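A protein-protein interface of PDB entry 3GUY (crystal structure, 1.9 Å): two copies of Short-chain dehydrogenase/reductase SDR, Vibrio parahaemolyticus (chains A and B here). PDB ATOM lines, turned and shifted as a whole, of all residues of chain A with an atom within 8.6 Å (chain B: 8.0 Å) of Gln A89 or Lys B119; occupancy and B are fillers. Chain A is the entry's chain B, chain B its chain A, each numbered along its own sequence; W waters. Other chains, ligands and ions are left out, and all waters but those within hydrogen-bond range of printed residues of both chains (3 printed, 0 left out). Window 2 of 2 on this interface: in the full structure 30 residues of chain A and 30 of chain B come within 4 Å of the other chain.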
ATOM      1  N   TYR A  84     -40.117   5.668 -24.942  1.00  0.00           N
ATOM      2  CA  TYR A  84     -39.156   6.187 -25.936  1.00  0.00           C
ATOM      3  C   TYR A  84     -37.772   5.860 -25.401  1.00  0.00           C
ATOM      4  O   TYR A  84     -37.497   6.084 -24.232  1.00  0.00           O
ATOM      5  CB  TYR A  84     -39.283   7.711 -26.165  1.00  0.00           C
ATOM      6  CG  TYR A  84     -38.322   8.240 -27.232  1.00  0.00           C
ATOM      7  CD1 TYR A  84     -38.388   7.773 -28.560  1.00  0.00           C
ATOM      8  CD2 TYR A  84     -37.358   9.189 -26.928  1.00  0.00           C
ATOM      9  CE1 TYR A  84     -37.525   8.226 -29.516  1.00  0.00           C
ATOM     10  CE2 TYR A  84     -36.510   9.690 -27.896  1.00  0.00           C
ATOM     11  CZ  TYR A  84     -36.578   9.189 -29.181  1.00  0.00           C
ATOM     12  OH  TYR A  84     -35.729   9.671 -30.111  1.00  0.00           O
ATOM     13  N   GLY A  86     -33.310   4.668 -26.180  1.00  0.00           N
ATOM     14  CA  GLY A  86     -32.063   4.888 -26.885  1.00  0.00           C
ATOM     15  C   GLY A  86     -31.065   5.635 -26.045  1.00  0.00           C
ATOM     16  O   GLY A  86     -31.423   6.400 -25.083  1.00  0.00           O
ATOM     17  N   LEU A  87     -29.796   5.467 -26.418  1.00  0.00           N
ATOM     18  CA  LEU A  87     -28.748   6.212 -25.792  1.00  0.00           C
ATOM     19  C   LEU A  87     -29.113   7.698 -25.862  1.00  0.00           C
ATOM     20  O   LEU A  87     -29.672   8.173 -26.860  1.00  0.00           O
ATOM     21  CB  LEU A  87     -27.400   5.940 -26.466  1.00  0.00           C
ATOM     22  CG  LEU A  87     -26.816   4.532 -26.319  1.00  0.00           C
ATOM     23  CD1 LEU A  87     -25.663   4.347 -27.294  1.00  0.00           C
ATOM     24  CD2 LEU A  87     -26.351   4.274 -24.872  1.00  0.00           C
ATOM     25  N   LEU A  88     -28.766   8.459 -24.826  1.00  0.00           N
ATOM     26  CA  LEU A  88     -29.301   9.822 -24.735  1.00  0.00           C
ATOM     27  C   LEU A  88     -28.902  10.663 -25.955  1.00  0.00           C
ATOM     28  O   LEU A  88     -29.715  11.437 -26.477  1.00  0.00           O
ATOM     29  CB  LEU A  88     -28.837  10.513 -23.444  1.00  0.00           C
ATOM     30  CG  LEU A  88     -29.334  11.951 -23.226  1.00  0.00           C
ATOM     31  CD1 LEU A  88     -30.840  12.212 -23.169  1.00  0.00           C
ATOM     32  CD2 LEU A  88     -28.710  12.474 -21.931  1.00  0.00           C
ATOM     33  N   GLN A  89     -27.657  10.533 -26.392  1.00  0.00           N
ATOM     34  CA  GLN A  89     -27.188  11.306 -27.577  1.00  0.00           C
ATOM     35  C   GLN A  89     -27.902  10.911 -28.916  1.00  0.00           C
ATOM     36  O   GLN A  89     -27.780  11.614 -29.913  1.00  0.00           O
ATOM     37  CB  GLN A  89     -25.655  11.225 -27.721  1.00  0.00           C
ATOM     38  CG  GLN A  89     -25.083   9.836 -28.199  1.00  0.00           C
ATOM     39  CD  GLN A  89     -24.921   8.821 -27.061  1.00  0.00           C
ATOM     40  OE1 GLN A  89     -25.508   8.965 -25.985  1.00  0.00           O
ATOM     41  NE2 GLN A  89     -24.107   7.812 -27.288  1.00  0.00           N
ATOM     42  N   GLU A  90     -28.583   9.781 -28.949  1.00  0.00           N
ATOM     43  CA  GLU A  90     -29.298   9.356 -30.160  1.00  0.00           C
ATOM     44  C   GLU A  90     -30.769   9.744 -30.076  1.00  0.00           C
ATOM     45  O   GLU A  90     -31.503   9.622 -31.070  1.00  0.00           O
ATOM     46  CB  GLU A  90     -29.216   7.847 -30.336  1.00  0.00           C
ATOM     47  CG  GLU A  90     -27.829   7.281 -30.171  1.00  0.00           C
ATOM     48  CD  GLU A  90     -27.145   6.933 -31.465  1.00  0.00           C
ATOM     49  OE1 GLU A  90     -27.683   7.260 -32.571  1.00  0.00           O
ATOM     50  OE2 GLU A  90     -26.046   6.305 -31.364  1.00  0.00           O
ATOM     51  N   GLN A  91     -31.219  10.183 -28.889  1.00  0.00           N
ATOM     52  CA  GLN A  91     -32.624  10.536 -28.730  1.00  0.00           C
ATOM     53  C   GLN A  91     -32.920  11.859 -29.407  1.00  0.00           C
ATOM     54  O   GLN A  91     -32.092  12.804 -29.381  1.00  0.00           O
ATOM     55  CB  GLN A  91     -32.990  10.595 -27.270  1.00  0.00           C
ATOM     56  CG  GLN A  91     -33.113   9.171 -26.696  1.00  0.00           C
ATOM     57  CD  GLN A  91     -33.719   9.150 -25.333  1.00  0.00           C
ATOM     58  OE1 GLN A  91     -34.379  10.117 -24.936  1.00  0.00           O
ATOM     59  NE2 GLN A  91     -33.598   7.997 -24.643  1.00  0.00           N
ATOM     60  N   ASP A  92     -34.099  11.917 -30.030  1.00  0.00           N
ATOM     61  CA  ASP A  92     -34.604  13.128 -30.685  1.00  0.00           C
ATOM     62  C   ASP A  92     -35.265  14.084 -29.677  1.00  0.00           C
ATOM     63  O   ASP A  92     -36.196  13.697 -28.991  1.00  0.00           O
ATOM     64  CB  ASP A  92     -35.659  12.711 -31.680  1.00  0.00           C
ATOM     65  CG  ASP A  92     -36.316  13.883 -32.398  1.00  0.00           C
ATOM     66  OD1 ASP A  92     -35.953  15.056 -32.172  1.00  0.00           O
ATOM     67  OD2 ASP A  92     -37.200  13.588 -33.243  1.00  0.00           O
ATOM     68  N   PRO A  93     -34.822  15.345 -29.619  1.00  0.00           N
ATOM     69  CA  PRO A  93     -35.372  16.185 -28.562  1.00  0.00           C
ATOM     70  C   PRO A  93     -36.889  16.427 -28.651  1.00  0.00           C
ATOM     71  O   PRO A  93     -37.518  16.649 -27.615  1.00  0.00           O
ATOM     72  CB  PRO A  93     -34.606  17.522 -28.746  1.00  0.00           C
ATOM     73  CG  PRO A  93     -33.278  17.067 -29.390  1.00  0.00           C
ATOM     74  CD  PRO A  93     -33.632  15.942 -30.266  1.00  0.00           C
ATOM     75  N   ILE A  96     -38.379  13.440 -26.947  1.00  0.00           N
ATOM     76  CA  ILE A  96     -38.188  13.669 -25.490  1.00  0.00           C
ATOM     77  C   ILE A  96     -39.320  14.591 -24.943  1.00  0.00           C
ATOM     78  O   ILE A  96     -39.916  14.312 -23.922  1.00  0.00           O
ATOM     79  CB  ILE A  96     -36.753  14.245 -25.133  1.00  0.00           C
ATOM     80  CG1 ILE A  96     -35.674  13.268 -25.569  1.00  0.00           C
ATOM     81  CG2 ILE A  96     -36.607  14.472 -23.597  1.00  0.00           C
ATOM     82  CD1 ILE A  96     -34.228  13.806 -25.545  1.00  0.00           C
ATOM     83  N   GLN A 139     -30.007   3.337 -21.838  1.00  0.00           N
ATOM     84  CA  GLN A 139     -30.884   3.491 -22.969  1.00  0.00           C
ATOM     85  C   GLN A 139     -32.311   3.872 -22.593  1.00  0.00           C
ATOM     86  O   GLN A 139     -33.166   3.871 -23.455  1.00  0.00           O
ATOM     87  CB  GLN A 139     -30.905   2.238 -23.872  1.00  0.00           C
ATOM     88  CG  GLN A 139     -29.484   1.698 -24.074  1.00  0.00           C
ATOM     89  CD  GLN A 139     -29.177   1.112 -25.430  1.00  0.00           C
ATOM     90  OE1 GLN A 139     -28.063   0.638 -25.615  1.00  0.00           O
ATOM     91  NE2 GLN A 139     -30.107   1.167 -26.384  1.00  0.00           N
ATOM     92  N   SER A 141     -32.762   6.718 -20.279  1.00  0.00           N
ATOM     93  CA  SER A 141     -32.519   7.867 -19.395  1.00  0.00           C
ATOM     94  C   SER A 141     -33.686   8.832 -19.238  1.00  0.00           C
ATOM     95  O   SER A 141     -34.012   9.195 -18.115  1.00  0.00           O
ATOM     96  CB  SER A 141     -31.245   8.592 -19.769  1.00  0.00           C
ATOM     97  OG  SER A 141     -31.279   9.197 -21.015  1.00  0.00           O
ATOM     98  N   THR A 142     -34.349   9.195 -20.334  1.00  0.00           N
ATOM     99  CA  THR A 142     -35.475  10.115 -20.299  1.00  0.00           C
ATOM    100  C   THR A 142     -36.745   9.461 -19.824  1.00  0.00           C
ATOM    101  O   THR A 142     -37.590  10.119 -19.202  1.00  0.00           O
ATOM    102  CB  THR A 142     -35.660  10.831 -21.635  1.00  0.00           C
ATOM    103  OG1 THR A 142     -35.793   9.878 -22.710  1.00  0.00           O
ATOM    104  CG2 THR A 142     -34.478  11.743 -21.907  1.00  0.00           C
ATOM    105  N   ILE B  72     -12.613  22.151 -25.817  1.00  0.00           N
ATOM    106  CA  ILE B  72     -13.290  21.086 -25.113  1.00  0.00           C
ATOM    107  C   ILE B  72     -13.261  21.505 -23.646  1.00  0.00           C
ATOM    108  O   ILE B  72     -12.196  21.610 -23.083  1.00  0.00           O
ATOM    109  CB  ILE B  72     -12.517  19.738 -25.305  1.00  0.00           C
ATOM    110  CG1 ILE B  72     -12.497  19.345 -26.785  1.00  0.00           C
ATOM    111  CG2 ILE B  72     -13.107  18.614 -24.440  1.00  0.00           C
ATOM    112  CD1 ILE B  72     -11.841  17.983 -27.060  1.00  0.00           C
ATOM    113  N   LEU B 111     -27.135  17.938 -20.716  1.00  0.00           N
ATOM    114  CA  LEU B 111     -26.458  16.678 -20.583  1.00  0.00           C
ATOM    115  C   LEU B 111     -26.469  15.942 -21.933  1.00  0.00           C
ATOM    116  O   LEU B 111     -25.452  15.327 -22.291  1.00  0.00           O
ATOM    117  CB  LEU B 111     -27.084  15.785 -19.503  1.00  0.00           C
ATOM    118  CG  LEU B 111     -26.310  14.518 -19.111  1.00  0.00           C
ATOM    119  CD1 LEU B 111     -24.855  14.881 -18.694  1.00  0.00           C
ATOM    120  CD2 LEU B 111     -27.046  13.745 -17.977  1.00  0.00           C
ATOM    121  N   ARG B 112     -27.576  15.978 -22.667  1.00  0.00           N
ATOM    122  CA  ARG B 112     -27.550  15.379 -23.993  1.00  0.00           C
ATOM    123  C   ARG B 112     -26.447  15.946 -24.945  1.00  0.00           C
ATOM    124  O   ARG B 112     -25.751  15.180 -25.668  1.00  0.00           O
ATOM    125  CB  ARG B 112     -28.899  15.518 -24.651  1.00  0.00           C
ATOM    126  CG  ARG B 112     -28.921  14.915 -26.005  1.00  0.00           C
ATOM    127  CD  ARG B 112     -30.346  14.817 -26.555  1.00  0.00           C
ATOM    128  NE  ARG B 112     -30.266  14.440 -27.963  1.00  0.00           N
ATOM    129  CZ  ARG B 112     -30.047  15.311 -28.953  1.00  0.00           C
ATOM    130  NH1 ARG B 112     -29.947  16.623 -28.721  1.00  0.00           N
ATOM    131  NH2 ARG B 112     -29.952  14.879 -30.183  1.00  0.00           N
ATOM    132  N   GLU B 113     -26.341  17.268 -24.999  1.00  0.00           N
ATOM    133  CA  GLU B 113     -25.340  17.903 -25.842  1.00  0.00           C
ATOM    134  C   GLU B 113     -23.927  17.553 -25.403  1.00  0.00           C
ATOM    135  O   GLU B 113     -23.030  17.385 -26.228  1.00  0.00           O
ATOM    136  CB  GLU B 113     -25.507  19.374 -25.768  1.00  0.00           C
ATOM    137  CG  GLU B 113     -24.822  20.144 -26.840  1.00  0.00           C
ATOM    138  CD  GLU B 113     -25.335  19.793 -28.228  1.00  0.00           C
ATOM    139  OE1 GLU B 113     -26.537  19.469 -28.390  1.00  0.00           O
ATOM    140  OE2 GLU B 113     -24.534  19.938 -29.166  1.00  0.00           O
ATOM    141  N   LEU B 114     -23.706  17.515 -24.096  1.00  0.00           N
ATOM    142  CA  LEU B 114     -22.425  17.123 -23.536  1.00  0.00           C
ATOM    143  C   LEU B 114     -22.013  15.701 -23.873  1.00  0.00           C
ATOM    144  O   LEU B 114     -20.878  15.493 -24.263  1.00  0.00           O
ATOM    145  CB  LEU B 114     -22.397  17.325 -22.023  1.00  0.00           C
ATOM    146  CG  LEU B 114     -22.501  18.763 -21.526  1.00  0.00           C
ATOM    147  CD1 LEU B 114     -22.506  18.757 -19.980  1.00  0.00           C
ATOM    148  CD2 LEU B 114     -21.399  19.687 -22.089  1.00  0.00           C
ATOM    149  N   VAL B 115     -22.918  14.736 -23.714  1.00  0.00           N
ATOM    150  CA  VAL B 115     -22.601  13.355 -24.030  1.00  0.00           C
ATOM    151  C   VAL B 115     -22.364  13.208 -25.542  1.00  0.00           C
ATOM    152  O   VAL B 115     -21.437  12.525 -25.970  1.00  0.00           O
ATOM    153  CB  VAL B 115     -23.666  12.359 -23.500  1.00  0.00           C
ATOM    154  CG1 VAL B 115     -23.504  10.951 -24.104  1.00  0.00           C
ATOM    155  CG2 VAL B 115     -23.606  12.256 -21.965  1.00  0.00           C
ATOM    156  N   LYS B 116     -23.198  13.870 -26.330  1.00  0.00           N
ATOM    157  CA  LYS B 116     -23.083  13.836 -27.787  1.00  0.00           C
ATOM    158  C   LYS B 116     -21.674  14.234 -28.242  1.00  0.00           C
ATOM    159  O   LYS B 116     -21.060  13.530 -29.006  1.00  0.00           O
ATOM    160  CB  LYS B 116     -24.100  14.802 -28.346  1.00  0.00           C
ATOM    161  CG  LYS B 116     -24.578  14.542 -29.687  1.00  0.00           C
ATOM    162  CD  LYS B 116     -25.756  15.431 -29.989  1.00  0.00           C
ATOM    163  CE  LYS B 116     -25.962  15.528 -31.467  1.00  0.00           C
ATOM    164  NZ  LYS B 116     -26.926  16.612 -31.794  1.00  0.00           N
ATOM    165  N   ARG B 117     -21.164  15.331 -27.701  1.00  0.00           N
ATOM    166  CA  ARG B 117     -19.922  15.926 -28.144  1.00  0.00           C
ATOM    167  C   ARG B 117     -18.696  15.438 -27.425  1.00  0.00           C
ATOM    168  O   ARG B 117     -17.623  15.453 -28.001  1.00  0.00           O
ATOM    169  CB  ARG B 117     -19.971  17.441 -27.927  1.00  0.00           C
ATOM    170  CG  ARG B 117     -20.953  18.184 -28.800  1.00  0.00           C
ATOM    171  CD  ARG B 117     -21.015  19.649 -28.435  1.00  0.00           C
ATOM    172  NE  ARG B 117     -21.952  20.311 -29.330  1.00  0.00           N
ATOM    173  CZ  ARG B 117     -21.642  20.866 -30.499  1.00  0.00           C
ATOM    174  NH1 ARG B 117     -20.386  20.880 -30.943  1.00  0.00           N
ATOM    175  NH2 ARG B 117     -22.615  21.415 -31.216  1.00  0.00           N
ATOM    176  N   TYR B 118     -18.829  15.140 -26.132  1.00  0.00           N
ATOM    177  CA  TYR B 118     -17.674  15.008 -25.231  1.00  0.00           C
ATOM    178  C   TYR B 118     -17.601  13.751 -24.358  1.00  0.00           C
ATOM    179  O   TYR B 118     -16.747  13.695 -23.463  1.00  0.00           O
ATOM    180  CB  TYR B 118     -17.590  16.184 -24.232  1.00  0.00           C
ATOM    181  CG  TYR B 118     -17.757  17.546 -24.786  1.00  0.00           C
ATOM    182  CD1 TYR B 118     -16.907  18.023 -25.797  1.00  0.00           C
ATOM    183  CD2 TYR B 118     -18.745  18.400 -24.289  1.00  0.00           C
ATOM    184  CE1 TYR B 118     -17.053  19.293 -26.312  1.00  0.00           C
ATOM    185  CE2 TYR B 118     -18.891  19.671 -24.788  1.00  0.00           C
ATOM    186  CZ  TYR B 118     -18.039  20.107 -25.803  1.00  0.00           C
ATOM    187  OH  TYR B 118     -18.184  21.360 -26.282  1.00  0.00           O
ATOM    188  N   LYS B 119     -18.467  12.769 -24.578  1.00  0.00           N
ATOM    189  CA  LYS B 119     -18.449  11.533 -23.758  1.00  0.00           C
ATOM    190  C   LYS B 119     -17.095  10.802 -23.788  1.00  0.00           C
ATOM    191  O   LYS B 119     -16.730  10.095 -22.822  1.00  0.00           O
ATOM    192  CB  LYS B 119     -19.570  10.578 -24.190  1.00  0.00           C
ATOM    193  CG  LYS B 119     -19.437  10.001 -25.594  1.00  0.00           C
ATOM    194  CD  LYS B 119     -20.656   9.172 -25.975  1.00  0.00           C
ATOM    195  CE  LYS B 119     -20.367   8.308 -27.222  1.00  0.00           C
ATOM    196  NZ  LYS B 119     -19.936   9.142 -28.352  1.00  0.00           N
ATOM    197  N   ASP B 120     -16.375  10.967 -24.904  1.00  0.00           N
ATOM    198  CA  ASP B 120     -15.051  10.366 -25.076  1.00  0.00           C
ATOM    199  C   ASP B 120     -13.913  11.300 -24.673  1.00  0.00           C
ATOM    200  O   ASP B 120     -12.765  11.064 -25.047  1.00  0.00           O
ATOM    201  CB  ASP B 120     -14.899   9.854 -26.519  1.00  0.00           C
ATOM    202  CG  ASP B 120     -15.950   8.810 -26.866  1.00  0.00           C
ATOM    203  OD1 ASP B 120     -16.053   7.787 -26.171  1.00  0.00           O
ATOM    204  OD2 ASP B 120     -16.725   9.023 -27.800  1.00  0.00           O
ATOM    205  N   GLN B 121     -14.219  12.342 -23.897  1.00  0.00           N
ATOM    206  CA  GLN B 121     -13.218  13.259 -23.362  1.00  0.00           C
ATOM    207  C   GLN B 121     -13.289  13.270 -21.847  1.00  0.00           C
ATOM    208  O   GLN B 121     -14.331  12.987 -21.289  1.00  0.00           O
ATOM    209  CB  GLN B 121     -13.459  14.677 -23.841  1.00  0.00           C
ATOM    210  CG  GLN B 121     -13.317  14.867 -25.343  1.00  0.00           C
ATOM    211  CD  GLN B 121     -11.895  14.644 -25.843  1.00  0.00           C
ATOM    212  OE1 GLN B 121     -10.911  14.720 -25.090  1.00  0.00           O
ATOM    213  NE2 GLN B 121     -11.788  14.367 -27.114  1.00  0.00           N
ATOM    214  N   PRO B 122     -12.172  13.577 -21.162  1.00  0.00           N
ATOM    215  CA  PRO B 122     -12.225  13.529 -19.680  1.00  0.00           C
ATOM    216  C   PRO B 122     -12.955  14.733 -19.028  1.00  0.00           C
ATOM    217  O   PRO B 122     -12.366  15.447 -18.209  1.00  0.00           O
ATOM    218  CB  PRO B 122     -10.739  13.499 -19.292  1.00  0.00           C
ATOM    219  CG  PRO B 122     -10.035  14.176 -20.423  1.00  0.00           C
ATOM    220  CD  PRO B 122     -10.769  13.612 -21.641  1.00  0.00           C
ATOM    221  N   VAL B 123     -14.219  14.951 -19.366  1.00  0.00           N
ATOM    222  CA  VAL B 123     -14.951  16.102 -18.856  1.00  0.00           C
ATOM    223  C   VAL B 123     -15.642  15.732 -17.518  1.00  0.00           C
ATOM    224  O   VAL B 123     -16.239  14.653 -17.401  1.00  0.00           O
ATOM    225  CB  VAL B 123     -16.017  16.642 -19.877  1.00  0.00           C
ATOM    226  CG1 VAL B 123     -16.641  17.965 -19.340  1.00  0.00           C
ATOM    227  CG2 VAL B 123     -15.409  16.840 -21.273  1.00  0.00           C
ATOM    228  N   VAL B 125     -18.676  16.557 -15.407  1.00  0.00           N
ATOM    229  CA  VAL B 125     -19.985  17.216 -15.507  1.00  0.00           C
ATOM    230  C   VAL B 125     -20.641  17.214 -14.145  1.00  0.00           C
ATOM    231  O   VAL B 125     -21.002  16.153 -13.629  1.00  0.00           O
ATOM    232  CB  VAL B 125     -20.856  16.486 -16.539  1.00  0.00           C
ATOM    233  CG1 VAL B 125     -22.273  17.105 -16.632  1.00  0.00           C
ATOM    234  CG2 VAL B 125     -20.149  16.498 -17.907  1.00  0.00           C
ATOM    235  N   VAL B 157     -27.674   7.879 -17.305  1.00  0.00           N
ATOM    236  CA  VAL B 157     -26.552   8.261 -18.145  1.00  0.00           C
ATOM    237  C   VAL B 157     -25.202   7.764 -17.579  1.00  0.00           C
ATOM    238  O   VAL B 157     -24.325   7.358 -18.359  1.00  0.00           O
ATOM    239  CB  VAL B 157     -26.529   9.785 -18.447  1.00  0.00           C
ATOM    240  CG1 VAL B 157     -25.334  10.144 -19.353  1.00  0.00           C
ATOM    241  CG2 VAL B 157     -27.827  10.214 -19.073  1.00  0.00           C
ATOM    242  N   GLU B 160     -24.689   4.457 -18.967  1.00  0.00           N
ATOM    243  CA  GLU B 160     -24.264   4.593 -20.397  1.00  0.00           C
ATOM    244  C   GLU B 160     -22.843   5.034 -20.564  1.00  0.00           C
ATOM    245  O   GLU B 160     -22.259   4.799 -21.606  1.00  0.00           O
ATOM    246  CB  GLU B 160     -25.145   5.567 -21.200  1.00  0.00           C
ATOM    247  CG  GLU B 160     -26.655   5.179 -21.184  1.00  0.00           C
ATOM    248  CD  GLU B 160     -27.586   6.119 -21.942  1.00  0.00           C
ATOM    249  OE1 GLU B 160     -27.128   7.119 -22.528  1.00  0.00           O
ATOM    250  OE2 GLU B 160     -28.802   5.845 -21.949  1.00  0.00           O
ATOM    251  N   LEU B 161     -22.321   5.753 -19.575  1.00  0.00           N
ATOM    252  CA  LEU B 161     -20.968   6.236 -19.605  1.00  0.00           C
ATOM    253  C   LEU B 161     -19.955   5.263 -19.035  1.00  0.00           C
ATOM    254  O   LEU B 161     -18.789   5.612 -18.956  1.00  0.00           O
ATOM    255  CB  LEU B 161     -20.847   7.583 -18.872  1.00  0.00           C
ATOM    256  CG  LEU B 161     -21.515   8.766 -19.517  1.00  0.00           C
ATOM    257  CD1 LEU B 161     -21.416  10.010 -18.653  1.00  0.00           C
ATOM    258  CD2 LEU B 161     -20.963   8.995 -20.936  1.00  0.00           C
ATOM    259  N   GLY B 163     -17.093   2.865 -18.672  1.00  0.00           N
ATOM    260  CA  GLY B 163     -15.956   2.630 -19.535  1.00  0.00           C
ATOM    261  C   GLY B 163     -15.578   3.824 -20.390  1.00  0.00           C
ATOM    262  O   GLY B 163     -14.723   3.681 -21.237  1.00  0.00           O
ATOM    263  N   LYS B 164     -16.216   4.990 -20.191  1.00  0.00           N
ATOM    264  CA  LYS B 164     -15.842   6.220 -20.907  1.00  0.00           C
ATOM    265  C   LYS B 164     -15.192   7.203 -19.956  1.00  0.00           C
ATOM    266  O   LYS B 164     -15.393   7.099 -18.760  1.00  0.00           O
ATOM    267  CB  LYS B 164     -17.071   6.825 -21.579  1.00  0.00           C
ATOM    268  CG  LYS B 164     -17.682   5.836 -22.563  1.00  0.00           C
ATOM    269  CD  LYS B 164     -18.301   6.509 -23.733  1.00  0.00           C
ATOM    270  CE  LYS B 164     -19.414   5.600 -24.282  1.00  0.00           C
ATOM    271  NZ  LYS B 164     -18.781   4.412 -24.889  1.00  0.00           N
ATOM    272  N   PRO B 165     -14.403   8.155 -20.464  1.00  0.00           N
ATOM    273  CA  PRO B 165     -13.771   9.065 -19.517  1.00  0.00           C
ATOM    274  C   PRO B 165     -14.642  10.168 -18.916  1.00  0.00           C
ATOM    275  O   PRO B 165     -14.261  10.690 -17.894  1.00  0.00           O
ATOM    276  CB  PRO B 165     -12.663   9.726 -20.354  1.00  0.00           C
ATOM    277  CG  PRO B 165     -13.143   9.591 -21.760  1.00  0.00           C
ATOM    278  CD  PRO B 165     -13.797   8.271 -21.804  1.00  0.00           C
ATOM    279  N   MET B 166     -15.739  10.553 -19.571  1.00  0.00           N
ATOM    280  CA  MET B 166     -16.621  11.585 -19.039  1.00  0.00           C
ATOM    281  C   MET B 166     -17.233  11.085 -17.733  1.00  0.00           C
ATOM    282  O   MET B 166     -17.795   9.952 -17.664  1.00  0.00           O
ATOM    283  CB  MET B 166     -17.753  11.943 -20.039  1.00  0.00           C
ATOM    284  CG  MET B 166     -18.775  12.948 -19.528  1.00  0.00           C
ATOM    285  SD  MET B 166     -20.011  13.492 -20.750  1.00  0.00           S
ATOM    286  CE  MET B 166     -21.358  13.724 -19.719  1.00  0.00           C
ATOM    287  N   LYS B 167     -17.190  11.938 -16.713  1.00  0.00           N
ATOM    288  CA  LYS B 167     -17.815  11.576 -15.420  1.00  0.00           C
ATOM    289  C   LYS B 167     -18.893  12.556 -15.008  1.00  0.00           C
ATOM    290  O   LYS B 167     -18.790  13.735 -15.276  1.00  0.00           O
ATOM    291  CB  LYS B 167     -16.763  11.533 -14.330  1.00  0.00           C
ATOM    292  CG  LYS B 167     -15.832  10.391 -14.509  1.00  0.00           C
ATOM    293  CD  LYS B 167     -14.924  10.203 -13.310  1.00  0.00           C
ATOM    294  CE  LYS B 167     -13.910  11.322 -13.178  1.00  0.00           C
ATOM    295  NZ  LYS B 167     -12.819  11.153 -14.164  1.00  0.00           N
HETATM  296  O   HOH W   1     -28.776  12.592 -31.932  1.00  0.00           O
HETATM  297  O   HOH W   2     -30.901   7.144 -22.472  1.00  0.00           O
HETATM  298  O   HOH W   3     -24.874   7.909 -23.416  1.00  0.00           O
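Printed residues of chain B within 4 Å of Leu A88: Arg B112 (3.4 Å), Val B157 (3.7 Å) and Glu B160 (3.1 Å).
Gln A89 touches just these residues of chain B: Arg B112, Val B115, Lys B116 and Lys B119.
Ile B72 touches none of the printed residues of chain A.
Printed residues of chain A within 4 Å of Lys B116: Gln A89 (3.7 Å).
No residue of chain A comes within 4 Å of Asp B120.
Printed residues of chain A within 4 Å of Val B157: Leu A88 and Ser A141.
Leu B161 touches none of the printed residues of chain A.
CD2 of Leu A87 touches CD of Glu B160 (3.7 Å).
Leu A88 touches Val B157.
Arg B112 touches Gln A89.
Gln A89 touches Val B115 (OE1 to CG1, 3.4 Å).
CA of Lys B116 touches CB of Gln A89, 3.7 Å away.
Lys B119 touches Gln A89 (CE to NE2, 3.8 Å).
Pro A93 touches Arg B112.
CB of Ser A141 touches CG2 of Val B157, at 3.8 Å.
The side-chain amino group (NZ) of Lys B119 lies within salt-bridge range of the side-chain carboxylate (OD2) of Asp B120, at 3.3 Å.
The backbone carbonyl oxygen (O) of Lys B119 sits at hydrogen-bond distance from the backbone NH (N) of Met B166 (3.4 Å).
The side-chain amide nitrogen (NE2) of Gln A91 lies within hydrogen-bond range of the backbone carbonyl oxygen (O) of Gly A86, 2.7 Å away.
The backbone carbonyl oxygen (O) of Gln A139 sits at hydrogen-bond distance from the backbone NH (N) of Gly A86 (2.8 Å).
OG1 of Thr A142 sits at hydrogen-bond distance from OE1 of Gln A91.
Water W1 bridges O of Gln A89 (2.5 Å) and NH2 of Arg B112 (3.1 Å).
Water W2 lies within hydrogen-bond range of OE2 of Glu B160, OG of Ser A141, O of Gly A86 and N of Leu A88.
Water W3 bridges OE1 of Glu B160 and OE1 of Gln A89.
No position is printed for both chains.
Of the 13 printed residues of chain A, 7 touch a printed residue of chain B.
Printed residues of chain A that touch a printed residue of chain B: Leu A87, Leu A88, Gln A89, Gln A91, Pro A93, Gln A139 and Ser A141.
Printed residues of chain B that touch a printed residue of chain A: Arg B112, Val B115, Lys B116, Lys B119, Val B157 and Glu B160.
Hydrophobic or aromatic side chains of chain B within 4 Å of the printed part of chain A: Val B115 and Val B157.
Among the printed residues, 12 pairs touch across the chains.
The backbone carbonyl oxygen (O) of Leu A88 lies within hydrogen-bond range of the guanidinium group (NE) of Arg B112, at 3.4 Å.
The guanidinium group of Arg B112 sits at hydrogen-bond distance from the backbone carbonyl oxygen of Gln A91 (2.8 Å).
OE1 of Glu B160 lies within hydrogen-bond range of N of Leu A88 (3.1 Å).
The side-chain carboxylate of Glu B160 sits at hydrogen-bond distance from the backbone NH of Gln A139 (2.8 Å).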
